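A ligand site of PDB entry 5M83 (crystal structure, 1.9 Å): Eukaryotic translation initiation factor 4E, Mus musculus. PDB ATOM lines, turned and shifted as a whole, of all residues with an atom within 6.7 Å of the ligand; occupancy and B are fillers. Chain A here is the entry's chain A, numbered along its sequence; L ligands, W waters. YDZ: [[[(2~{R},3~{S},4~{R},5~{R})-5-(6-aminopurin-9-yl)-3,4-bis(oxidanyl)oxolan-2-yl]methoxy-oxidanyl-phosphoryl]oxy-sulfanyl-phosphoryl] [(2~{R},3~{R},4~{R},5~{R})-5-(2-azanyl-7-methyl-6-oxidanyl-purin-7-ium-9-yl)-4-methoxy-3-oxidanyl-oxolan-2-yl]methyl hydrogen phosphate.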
ATOM      1  N   PHE A  21       0.468  -9.139  16.608  1.00  0.00           N
ATOM      2  CA  PHE A  21       1.850  -9.024  16.158  1.00  0.00           C
ATOM      3  C   PHE A  21       2.121 -10.194  15.244  1.00  0.00           C
ATOM      4  O   PHE A  21       1.776 -11.331  15.586  1.00  0.00           O
ATOM      5  CB  PHE A  21       2.831  -9.005  17.343  1.00  0.00           C
ATOM      6  CG  PHE A  21       4.291  -9.005  16.934  1.00  0.00           C
ATOM      7  CD1 PHE A  21       4.969 -10.204  16.713  1.00  0.00           C
ATOM      8  CD2 PHE A  21       4.992  -7.824  16.792  1.00  0.00           C
ATOM      9  CE1 PHE A  21       6.293 -10.213  16.347  1.00  0.00           C
ATOM     10  CE2 PHE A  21       6.342  -7.831  16.402  1.00  0.00           C
ATOM     11  CZ  PHE A  21       6.977  -9.042  16.195  1.00  0.00           C
ATOM     12  N   TRP A  29      10.257  -4.179  14.857  1.00  0.00           N
ATOM     13  CA  TRP A  29       9.366  -4.818  15.795  1.00  0.00           C
ATOM     14  C   TRP A  29       8.112  -3.972  16.004  1.00  0.00           C
ATOM     15  O   TRP A  29       6.985  -4.491  15.944  1.00  0.00           O
ATOM     16  CB  TRP A  29      10.080  -5.058  17.136  1.00  0.00           C
ATOM     17  CG  TRP A  29       9.170  -5.758  18.127  1.00  0.00           C
ATOM     18  CD1 TRP A  29       9.034  -7.104  18.297  1.00  0.00           C
ATOM     19  CD2 TRP A  29       8.279  -5.138  19.071  1.00  0.00           C
ATOM     20  NE1 TRP A  29       8.088  -7.359  19.283  1.00  0.00           N
ATOM     21  CE2 TRP A  29       7.626  -6.172  19.770  1.00  0.00           C
ATOM     22  CE3 TRP A  29       7.975  -3.808  19.394  1.00  0.00           C
ATOM     23  CZ2 TRP A  29       6.684  -5.920  20.759  1.00  0.00           C
ATOM     24  CZ3 TRP A  29       7.040  -3.555  20.391  1.00  0.00           C
ATOM     25  CH2 TRP A  29       6.400  -4.612  21.054  1.00  0.00           C
ATOM     26  N   GLN A  30       8.282  -2.680  16.231  1.00  0.00           N
ATOM     27  CA  GLN A  30       7.111  -1.818  16.416  1.00  0.00           C
ATOM     28  C   GLN A  30       6.203  -1.836  15.192  1.00  0.00           C
ATOM     29  O   GLN A  30       4.976  -1.775  15.329  1.00  0.00           O
ATOM     30  CB  GLN A  30       7.543  -0.395  16.754  1.00  0.00           C
ATOM     31  CG  GLN A  30       8.175  -0.226  18.123  1.00  0.00           C
ATOM     32  N   GLY A  61       5.541 -17.113  15.877  1.00  0.00           N
ATOM     33  CA  GLY A  61       6.030 -15.754  15.766  1.00  0.00           C
ATOM     34  C   GLY A  61       4.960 -14.699  15.968  1.00  0.00           C
ATOM     35  O   GLY A  61       5.278 -13.503  15.968  1.00  0.00           O
ATOM     36  N   ASP A  63       1.737 -12.798  18.138  1.00  0.00           N
ATOM     37  CA  ASP A  63       1.321 -12.495  19.498  1.00  0.00           C
ATOM     38  C   ASP A  63      -0.087 -11.937  19.454  1.00  0.00           C
ATOM     39  O   ASP A  63      -0.486 -11.311  18.476  1.00  0.00           O
ATOM     40  CB  ASP A  63       2.150 -11.394  20.256  1.00  0.00           C
ATOM     41  CG  ASP A  63       3.622 -11.542  20.155  1.00  0.00           C
ATOM     42  OD1 ASP A  63       4.134 -12.665  20.007  1.00  0.00           O
ATOM     43  OD2 ASP A  63       4.316 -10.490  20.297  1.00  0.00           O
ATOM     44  N   PRO A  73       1.096  -2.104  23.915  1.00  0.00           N
ATOM     45  CA  PRO A  73       1.726  -3.298  24.510  1.00  0.00           C
ATOM     46  C   PRO A  73       3.230  -3.366  24.261  1.00  0.00           C
ATOM     47  O   PRO A  73       3.765  -4.345  23.704  1.00  0.00           O
ATOM     48  CB  PRO A  73       0.946  -4.436  23.835  1.00  0.00           C
ATOM     49  CG  PRO A  73       0.595  -3.891  22.488  1.00  0.00           C
ATOM     50  CD  PRO A  73       0.426  -2.401  22.640  1.00  0.00           C
ATOM     51  N   MET A  74       3.924  -2.332  24.703  1.00  0.00           N
ATOM     52  CA  MET A  74       5.366  -2.256  24.556  1.00  0.00           C
ATOM     53  C   MET A  74       5.955  -1.603  25.799  1.00  0.00           C
ATOM     54  O   MET A  74       5.302  -0.820  26.490  1.00  0.00           O
ATOM     55  CB  MET A  74       5.775  -1.465  23.314  1.00  0.00           C
ATOM     56  CG  MET A  74       5.296  -0.029  23.333  1.00  0.00           C
ATOM     57  SD  MET A  74       5.687   0.854  21.808  1.00  0.00           S
ATOM     58  CE  MET A  74       4.566   0.078  20.670  1.00  0.00           C
ATOM     59  N   TRP A  75       7.200  -1.976  26.098  1.00  0.00           N
ATOM     60  CA  TRP A  75       7.888  -1.491  27.290  1.00  0.00           C
ATOM     61  C   TRP A  75       7.916   0.018  27.370  1.00  0.00           C
ATOM     62  O   TRP A  75       7.983   0.572  28.462  1.00  0.00           O
ATOM     63  CB  TRP A  75       9.338  -1.986  27.327  1.00  0.00           C
ATOM     64  CG  TRP A  75       9.487  -3.454  27.204  1.00  0.00           C
ATOM     65  CD1 TRP A  75       8.693  -4.409  27.762  1.00  0.00           C
ATOM     66  CD2 TRP A  75      10.509  -4.147  26.478  1.00  0.00           C
ATOM     67  NE1 TRP A  75       9.162  -5.660  27.439  1.00  0.00           N
ATOM     68  CE2 TRP A  75      10.274  -5.526  26.648  1.00  0.00           C
ATOM     69  CE3 TRP A  75      11.590  -3.736  25.701  1.00  0.00           C
ATOM     70  CZ2 TRP A  75      11.079  -6.492  26.062  1.00  0.00           C
ATOM     71  CZ3 TRP A  75      12.392  -4.711  25.119  1.00  0.00           C
ATOM     72  CH2 TRP A  75      12.130  -6.069  25.310  1.00  0.00           C
ATOM     73  N   GLU A  76       7.906   0.686  26.225  1.00  0.00           N
ATOM     74  CA  GLU A  76       8.194   2.111  26.190  1.00  0.00           C
ATOM     75  C   GLU A  76       7.014   2.955  26.645  1.00  0.00           C
ATOM     76  O   GLU A  76       7.192   4.140  26.948  1.00  0.00           O
ATOM     77  CB  GLU A  76       8.628   2.527  24.777  1.00  0.00           C
ATOM     78  CG  GLU A  76       9.909   1.877  24.244  1.00  0.00           C
ATOM     79  CD  GLU A  76       9.717   0.494  23.644  1.00  0.00           C
ATOM     80  OE1 GLU A  76      10.568   0.102  22.825  1.00  0.00           O
ATOM     81  OE2 GLU A  76       8.739  -0.190  23.989  1.00  0.00           O
ATOM     82  N   ARG A  85       6.213  -8.137  34.390  1.00  0.00           N
ATOM     83  CA  ARG A  85       5.195  -9.083  33.997  1.00  0.00           C
ATOM     84  C   ARG A  85       5.278 -10.344  34.850  1.00  0.00           C
ATOM     85  O   ARG A  85       6.371 -10.762  35.226  1.00  0.00           O
ATOM     86  CB  ARG A  85       5.325  -9.457  32.511  1.00  0.00           C
ATOM     87  CG  ARG A  85       6.563 -10.301  32.222  1.00  0.00           C
ATOM     88  CD  ARG A  85       6.875 -10.342  30.741  1.00  0.00           C
ATOM     89  NE  ARG A  85       8.151 -11.028  30.516  1.00  0.00           N
ATOM     90  CZ  ARG A  85       8.468 -11.678  29.404  1.00  0.00           C
ATOM     91  NH1 ARG A  85       7.618 -11.744  28.392  1.00  0.00           N
ATOM     92  NH2 ARG A  85       9.663 -12.255  29.291  1.00  0.00           N
ATOM     93  N   VAL A 126      -0.181 -10.595  27.417  1.00  0.00           N
ATOM     94  CA  VAL A 126       0.398 -10.898  26.112  1.00  0.00           C
ATOM     95  C   VAL A 126       0.521 -12.399  26.044  1.00  0.00           C
ATOM     96  O   VAL A 126       0.880 -13.023  27.044  1.00  0.00           O
ATOM     97  CB  VAL A 126       1.787 -10.245  25.902  1.00  0.00           C
ATOM     98  CG1 VAL A 126       2.330 -10.570  24.498  1.00  0.00           C
ATOM     99  CG2 VAL A 126       1.737  -8.717  26.130  1.00  0.00           C
ATOM    100  N   ASN A 128       2.607 -15.040  23.545  1.00  0.00           N
ATOM    101  CA  ASN A 128       3.562 -15.228  22.454  1.00  0.00           C
ATOM    102  C   ASN A 128       3.487 -16.676  22.028  1.00  0.00           C
ATOM    103  O   ASN A 128       3.686 -17.575  22.847  1.00  0.00           O
ATOM    104  CB  ASN A 128       4.991 -14.882  22.875  1.00  0.00           C
ATOM    105  CG  ASN A 128       5.095 -13.575  23.661  1.00  0.00           C
ATOM    106  OD1 ASN A 128       5.339 -13.580  24.877  1.00  0.00           O
ATOM    107  ND2 ASN A 128       4.907 -12.473  22.979  1.00  0.00           N
ATOM    108  N   VAL A 129       3.162 -16.908  20.770  1.00  0.00           N
ATOM    109  CA  VAL A 129       3.132 -18.226  20.163  1.00  0.00           C
ATOM    110  C   VAL A 129       4.468 -18.416  19.461  1.00  0.00           C
ATOM    111  O   VAL A 129       4.797 -17.657  18.524  1.00  0.00           O
ATOM    112  CB  VAL A 129       1.953 -18.328  19.183  1.00  0.00           C
ATOM    113  CG1 VAL A 129       1.926 -19.675  18.496  1.00  0.00           C
ATOM    114  CG2 VAL A 129       0.650 -18.066  19.914  1.00  0.00           C
ATOM    115  N   ARG A 130       5.251 -19.424  19.903  1.00  0.00           N
ATOM    116  CA  ARG A 130       6.626 -19.603  19.447  1.00  0.00           C
ATOM    117  C   ARG A 130       6.932 -21.086  19.293  1.00  0.00           C
ATOM    118  O   ARG A 130       6.527 -21.900  20.130  1.00  0.00           O
ATOM    119  CB  ARG A 130       7.643 -19.018  20.450  1.00  0.00           C
ATOM    120  CG  ARG A 130       7.677 -17.505  20.591  1.00  0.00           C
ATOM    121  CD  ARG A 130       7.923 -16.759  19.299  1.00  0.00           C
ATOM    122  NE  ARG A 130       7.958 -15.314  19.639  1.00  0.00           N
ATOM    123  CZ  ARG A 130       6.904 -14.510  19.578  1.00  0.00           C
ATOM    124  NH1 ARG A 130       5.743 -14.978  19.163  1.00  0.00           N
ATOM    125  NH2 ARG A 130       7.021 -13.235  19.923  1.00  0.00           N
ATOM    126  N   GLY A 133       8.565 -22.676  22.387  1.00  0.00           N
ATOM    127  CA  GLY A 133       7.796 -22.671  23.608  1.00  0.00           C
ATOM    128  C   GLY A 133       6.993 -21.394  23.726  1.00  0.00           C
ATOM    129  O   GLY A 133       7.525 -20.305  23.480  1.00  0.00           O
ATOM    130  N   ASP A 134       5.718 -21.509  24.067  1.00  0.00           N
ATOM    131  CA  ASP A 134       4.856 -20.329  24.130  1.00  0.00           C
ATOM    132  C   ASP A 134       4.981 -19.622  25.486  1.00  0.00           C
ATOM    133  O   ASP A 134       5.486 -20.170  26.465  1.00  0.00           O
ATOM    134  CB  ASP A 134       3.401 -20.719  23.888  1.00  0.00           C
ATOM    135  CG  ASP A 134       3.216 -21.481  22.567  1.00  0.00           C
ATOM    136  OD1 ASP A 134       3.777 -21.071  21.528  1.00  0.00           O
ATOM    137  OD2 ASP A 134       2.462 -22.466  22.565  1.00  0.00           O
ATOM    138  N   LYS A 135       4.485 -18.377  25.535  1.00  0.00           N
ATOM    139  CA  LYS A 135       4.513 -17.611  26.766  1.00  0.00           C
ATOM    140  C   LYS A 135       3.216 -16.843  26.903  1.00  0.00           C
ATOM    141  O   LYS A 135       2.692 -16.342  25.907  1.00  0.00           O
ATOM    142  CB  LYS A 135       5.666 -16.599  26.797  1.00  0.00           C
ATOM    143  CG  LYS A 135       7.044 -17.202  26.848  1.00  0.00           C
ATOM    144  CD  LYS A 135       8.077 -16.081  26.864  1.00  0.00           C
ATOM    145  CE  LYS A 135       9.487 -16.626  26.768  1.00  0.00           C
ATOM    146  NZ  LYS A 135       9.821 -16.998  25.370  1.00  0.00           N
ATOM    147  N   TRP A 139       1.086  -7.996  32.410  1.00  0.00           N
ATOM    148  CA  TRP A 139       1.921  -6.826  32.638  1.00  0.00           C
ATOM    149  C   TRP A 139       1.293  -5.889  33.664  1.00  0.00           C
ATOM    150  O   TRP A 139       0.092  -5.576  33.591  1.00  0.00           O
ATOM    151  CB  TRP A 139       2.127  -6.046  31.336  1.00  0.00           C
ATOM    152  CG  TRP A 139       2.941  -6.743  30.296  1.00  0.00           C
ATOM    153  CD1 TRP A 139       3.149  -8.106  30.145  1.00  0.00           C
ATOM    154  CD2 TRP A 139       3.716  -6.112  29.276  1.00  0.00           C
ATOM    155  NE1 TRP A 139       3.981  -8.342  29.077  1.00  0.00           N
ATOM    156  CE2 TRP A 139       4.338  -7.125  28.523  1.00  0.00           C
ATOM    157  CE3 TRP A 139       3.918  -4.775  28.898  1.00  0.00           C
ATOM    158  CZ2 TRP A 139       5.177  -6.837  27.426  1.00  0.00           C
ATOM    159  CZ3 TRP A 139       4.737  -4.500  27.807  1.00  0.00           C
ATOM    160  CH2 TRP A 139       5.360  -5.517  27.096  1.00  0.00           C
ATOM    161  N   THR A 176      14.354  -7.102  31.189  1.00  0.00           N
ATOM    162  CA  THR A 176      14.084  -7.889  29.990  1.00  0.00           C
ATOM    163  C   THR A 176      14.678  -7.255  28.738  1.00  0.00           C
ATOM    164  O   THR A 176      15.163  -7.955  27.848  1.00  0.00           O
ATOM    165  CB  THR A 176      12.582  -8.071  29.826  1.00  0.00           C
ATOM    166  OG1 THR A 176      12.013  -8.536  31.058  1.00  0.00           O
ATOM    167  CG2 THR A 176      12.281  -9.079  28.728  1.00  0.00           C
ATOM    168  N   ALA A 177      14.651  -5.923  28.677  1.00  0.00           N
ATOM    169  CA  ALA A 177      15.053  -5.175  27.487  1.00  0.00           C
ATOM    170  C   ALA A 177      16.553  -5.151  27.255  1.00  0.00           C
ATOM    171  O   ALA A 177      16.993  -4.711  26.184  1.00  0.00           O
ATOM    172  CB  ALA A 177      14.538  -3.742  27.593  1.00  0.00           C
HETATM  173  C1  YDZ L   1      10.621  -3.003  21.944  1.00  0.00           C
HETATM  174  C2  YDZ L   1       9.764  -7.349  22.294  1.00  0.00           C
HETATM  175  C3  YDZ L   1      10.434  -5.318  21.894  1.00  0.00           C
HETATM  176  C4  YDZ L   1       9.421  -5.278  22.830  1.00  0.00           C
HETATM  177  C5  YDZ L   1       9.002  -4.043  23.325  1.00  0.00           C
HETATM  178  O4  YDZ L   1      12.179 -14.291  25.137  1.00  0.00           O
HETATM  179  P1  YDZ L   1      12.893 -14.668  23.736  1.00  0.00           P
HETATM  180  O5  YDZ L   1      13.848 -15.819  23.949  1.00  0.00           O
HETATM  181  O6  YDZ L   1      13.650 -13.457  23.241  1.00  0.00           O
HETATM  182  O7  YDZ L   1      11.801 -15.133  22.634  1.00  0.00           O
HETATM  183  P2  YDZ L   1      10.480 -14.296  22.241  1.00  0.00           P
HETATM  184  O8  YDZ L   1      10.227 -14.390  20.790  1.00  0.00           O
HETATM  185  S1  YDZ L   1       8.830 -15.018  23.239  1.00  0.00           S
HETATM  186  O9  YDZ L   1      10.724 -12.780  22.721  1.00  0.00           O
HETATM  187  P3  YDZ L   1       9.807 -11.504  22.359  1.00  0.00           P
HETATM  188  O10 YDZ L   1       8.963 -11.121  23.552  1.00  0.00           O
HETATM  189  O11 YDZ L   1       9.092 -11.709  21.070  1.00  0.00           O
HETATM  190  O12 YDZ L   1      10.892 -10.346  22.106  1.00  0.00           O
HETATM  191  C16 YDZ L   1      11.882 -10.593  21.114  1.00  0.00           C
HETATM  192  C17 YDZ L   1      12.434  -9.232  20.743  1.00  0.00           C
HETATM  193  O13 YDZ L   1      11.383  -8.403  20.229  1.00  0.00           O
HETATM  194  C18 YDZ L   1      12.952  -8.485  21.955  1.00  0.00           C
HETATM  195  O14 YDZ L   1      14.248  -8.956  22.357  1.00  0.00           O
HETATM  196  C19 YDZ L   1      12.930  -7.060  21.414  1.00  0.00           C
HETATM  197  O15 YDZ L   1      14.023  -6.863  20.521  1.00  0.00           O
HETATM  198  C20 YDZ L   1      14.016  -5.574  19.906  1.00  0.00           C
HETATM  199  C21 YDZ L   1      11.642  -7.052  20.624  1.00  0.00           C
HETATM  200  N6  YDZ L   1      10.613  -6.591  21.566  1.00  0.00           N
HETATM  201  N7  YDZ L   1       9.017  -6.553  23.081  1.00  0.00           N
HETATM  202  C22 YDZ L   1       7.965  -7.077  23.985  1.00  0.00           C
HETATM  203  N8  YDZ L   1      11.022  -4.191  21.457  1.00  0.00           N
HETATM  204  N9  YDZ L   1      11.232  -1.877  21.498  1.00  0.00           N
HETATM  205  N10 YDZ L   1       9.634  -2.933  22.864  1.00  0.00           N
HETATM  206  O16 YDZ L   1       8.020  -3.877  24.254  1.00  0.00           O
HETATM  207  O   HOH W   1      10.472 -10.094  25.578  1.00  0.00           O
HETATM  208  O   HOH W   2       7.882 -12.456  25.373  1.00  0.00           O
HETATM  209  O   HOH W   3       6.839  -9.721  20.604  1.00  0.00           O
HETATM  210  O   HOH W   4       5.442  -9.251  23.232  1.00  0.00           O
HETATM  211  O   HOH W   5       9.340 -11.158  18.220  1.00  0.00           O
HETATM  212  O   HOH W   6       6.555  -9.816  25.711  1.00  0.00           O
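Water W2 lies within hydrogen-bond range of O10 of the ligand (2.5 Å), OD1 of Asn 128 (2.8 Å) and NH1 of Arg 85 (3.1 Å). Water W3 lies within hydrogen-bond range of the side-chain carboxylate (OD2) of Asp 63 (2.7 Å), the indole nitrogen (NE1) of Trp 29 (3.0 Å) and an oxygen (O11) of the ligand (3.0 Å). Water W4 lies within hydrogen-bond range of ND2 of Asn 128 (3.3 Å) and OD2 of Asp 63 (3.4 Å). Water W6 bridges the guanidinium group of Arg 85 (3.5 Å) and an oxygen (O10) of the ligand (3.5 Å).
The side-chain carboxylate (OD1) of Asp 134 is in hydrogen-bond range of the backbone NH (N) of Arg 130 (2.7 Å). NH1 of Arg 130 lies within salt-bridge range of OD1 of Asp 63, at 2.9 Å. ND2 of Asn 128 sits at hydrogen-bond distance from OD1 of Asp 63 (3.1 Å). The backbone NH (N) of Asn 128 lies within hydrogen-bond range of the backbone carbonyl oxygen (O) of Lys 135, 2.7 Å away.
N9 of the ligand lies within hydrogen-bond range of OE1 of Glu 76 (2.5 Å). NZ of Lys 135 lies within salt-bridge range of O4 of the ligand (3.6 Å). The backbone NH of Trp 75 sits at hydrogen-bond distance from an oxygen (O16) of the ligand, 2.8 Å away. The guanidinium group of Arg 130 lies within salt-bridge range of an oxygen (O11) of the ligand, at 2.8 Å.
The indole nitrogen of Trp 29 lies close to a nitrogen (N6) of the ligand, at 3.5 Å. Residues that only touch the ligand: Met 74 (3.1 Å) and Asn 128 (3.9 Å). Hydrophobic or aromatic side chains that line the ligand: Trp 29, Met 74 and Trp 75. Within 4 Å of the ligand: Trp 29, Met 74, Trp 75, Glu 76, Asn 128, Arg 130 and Lys 135.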
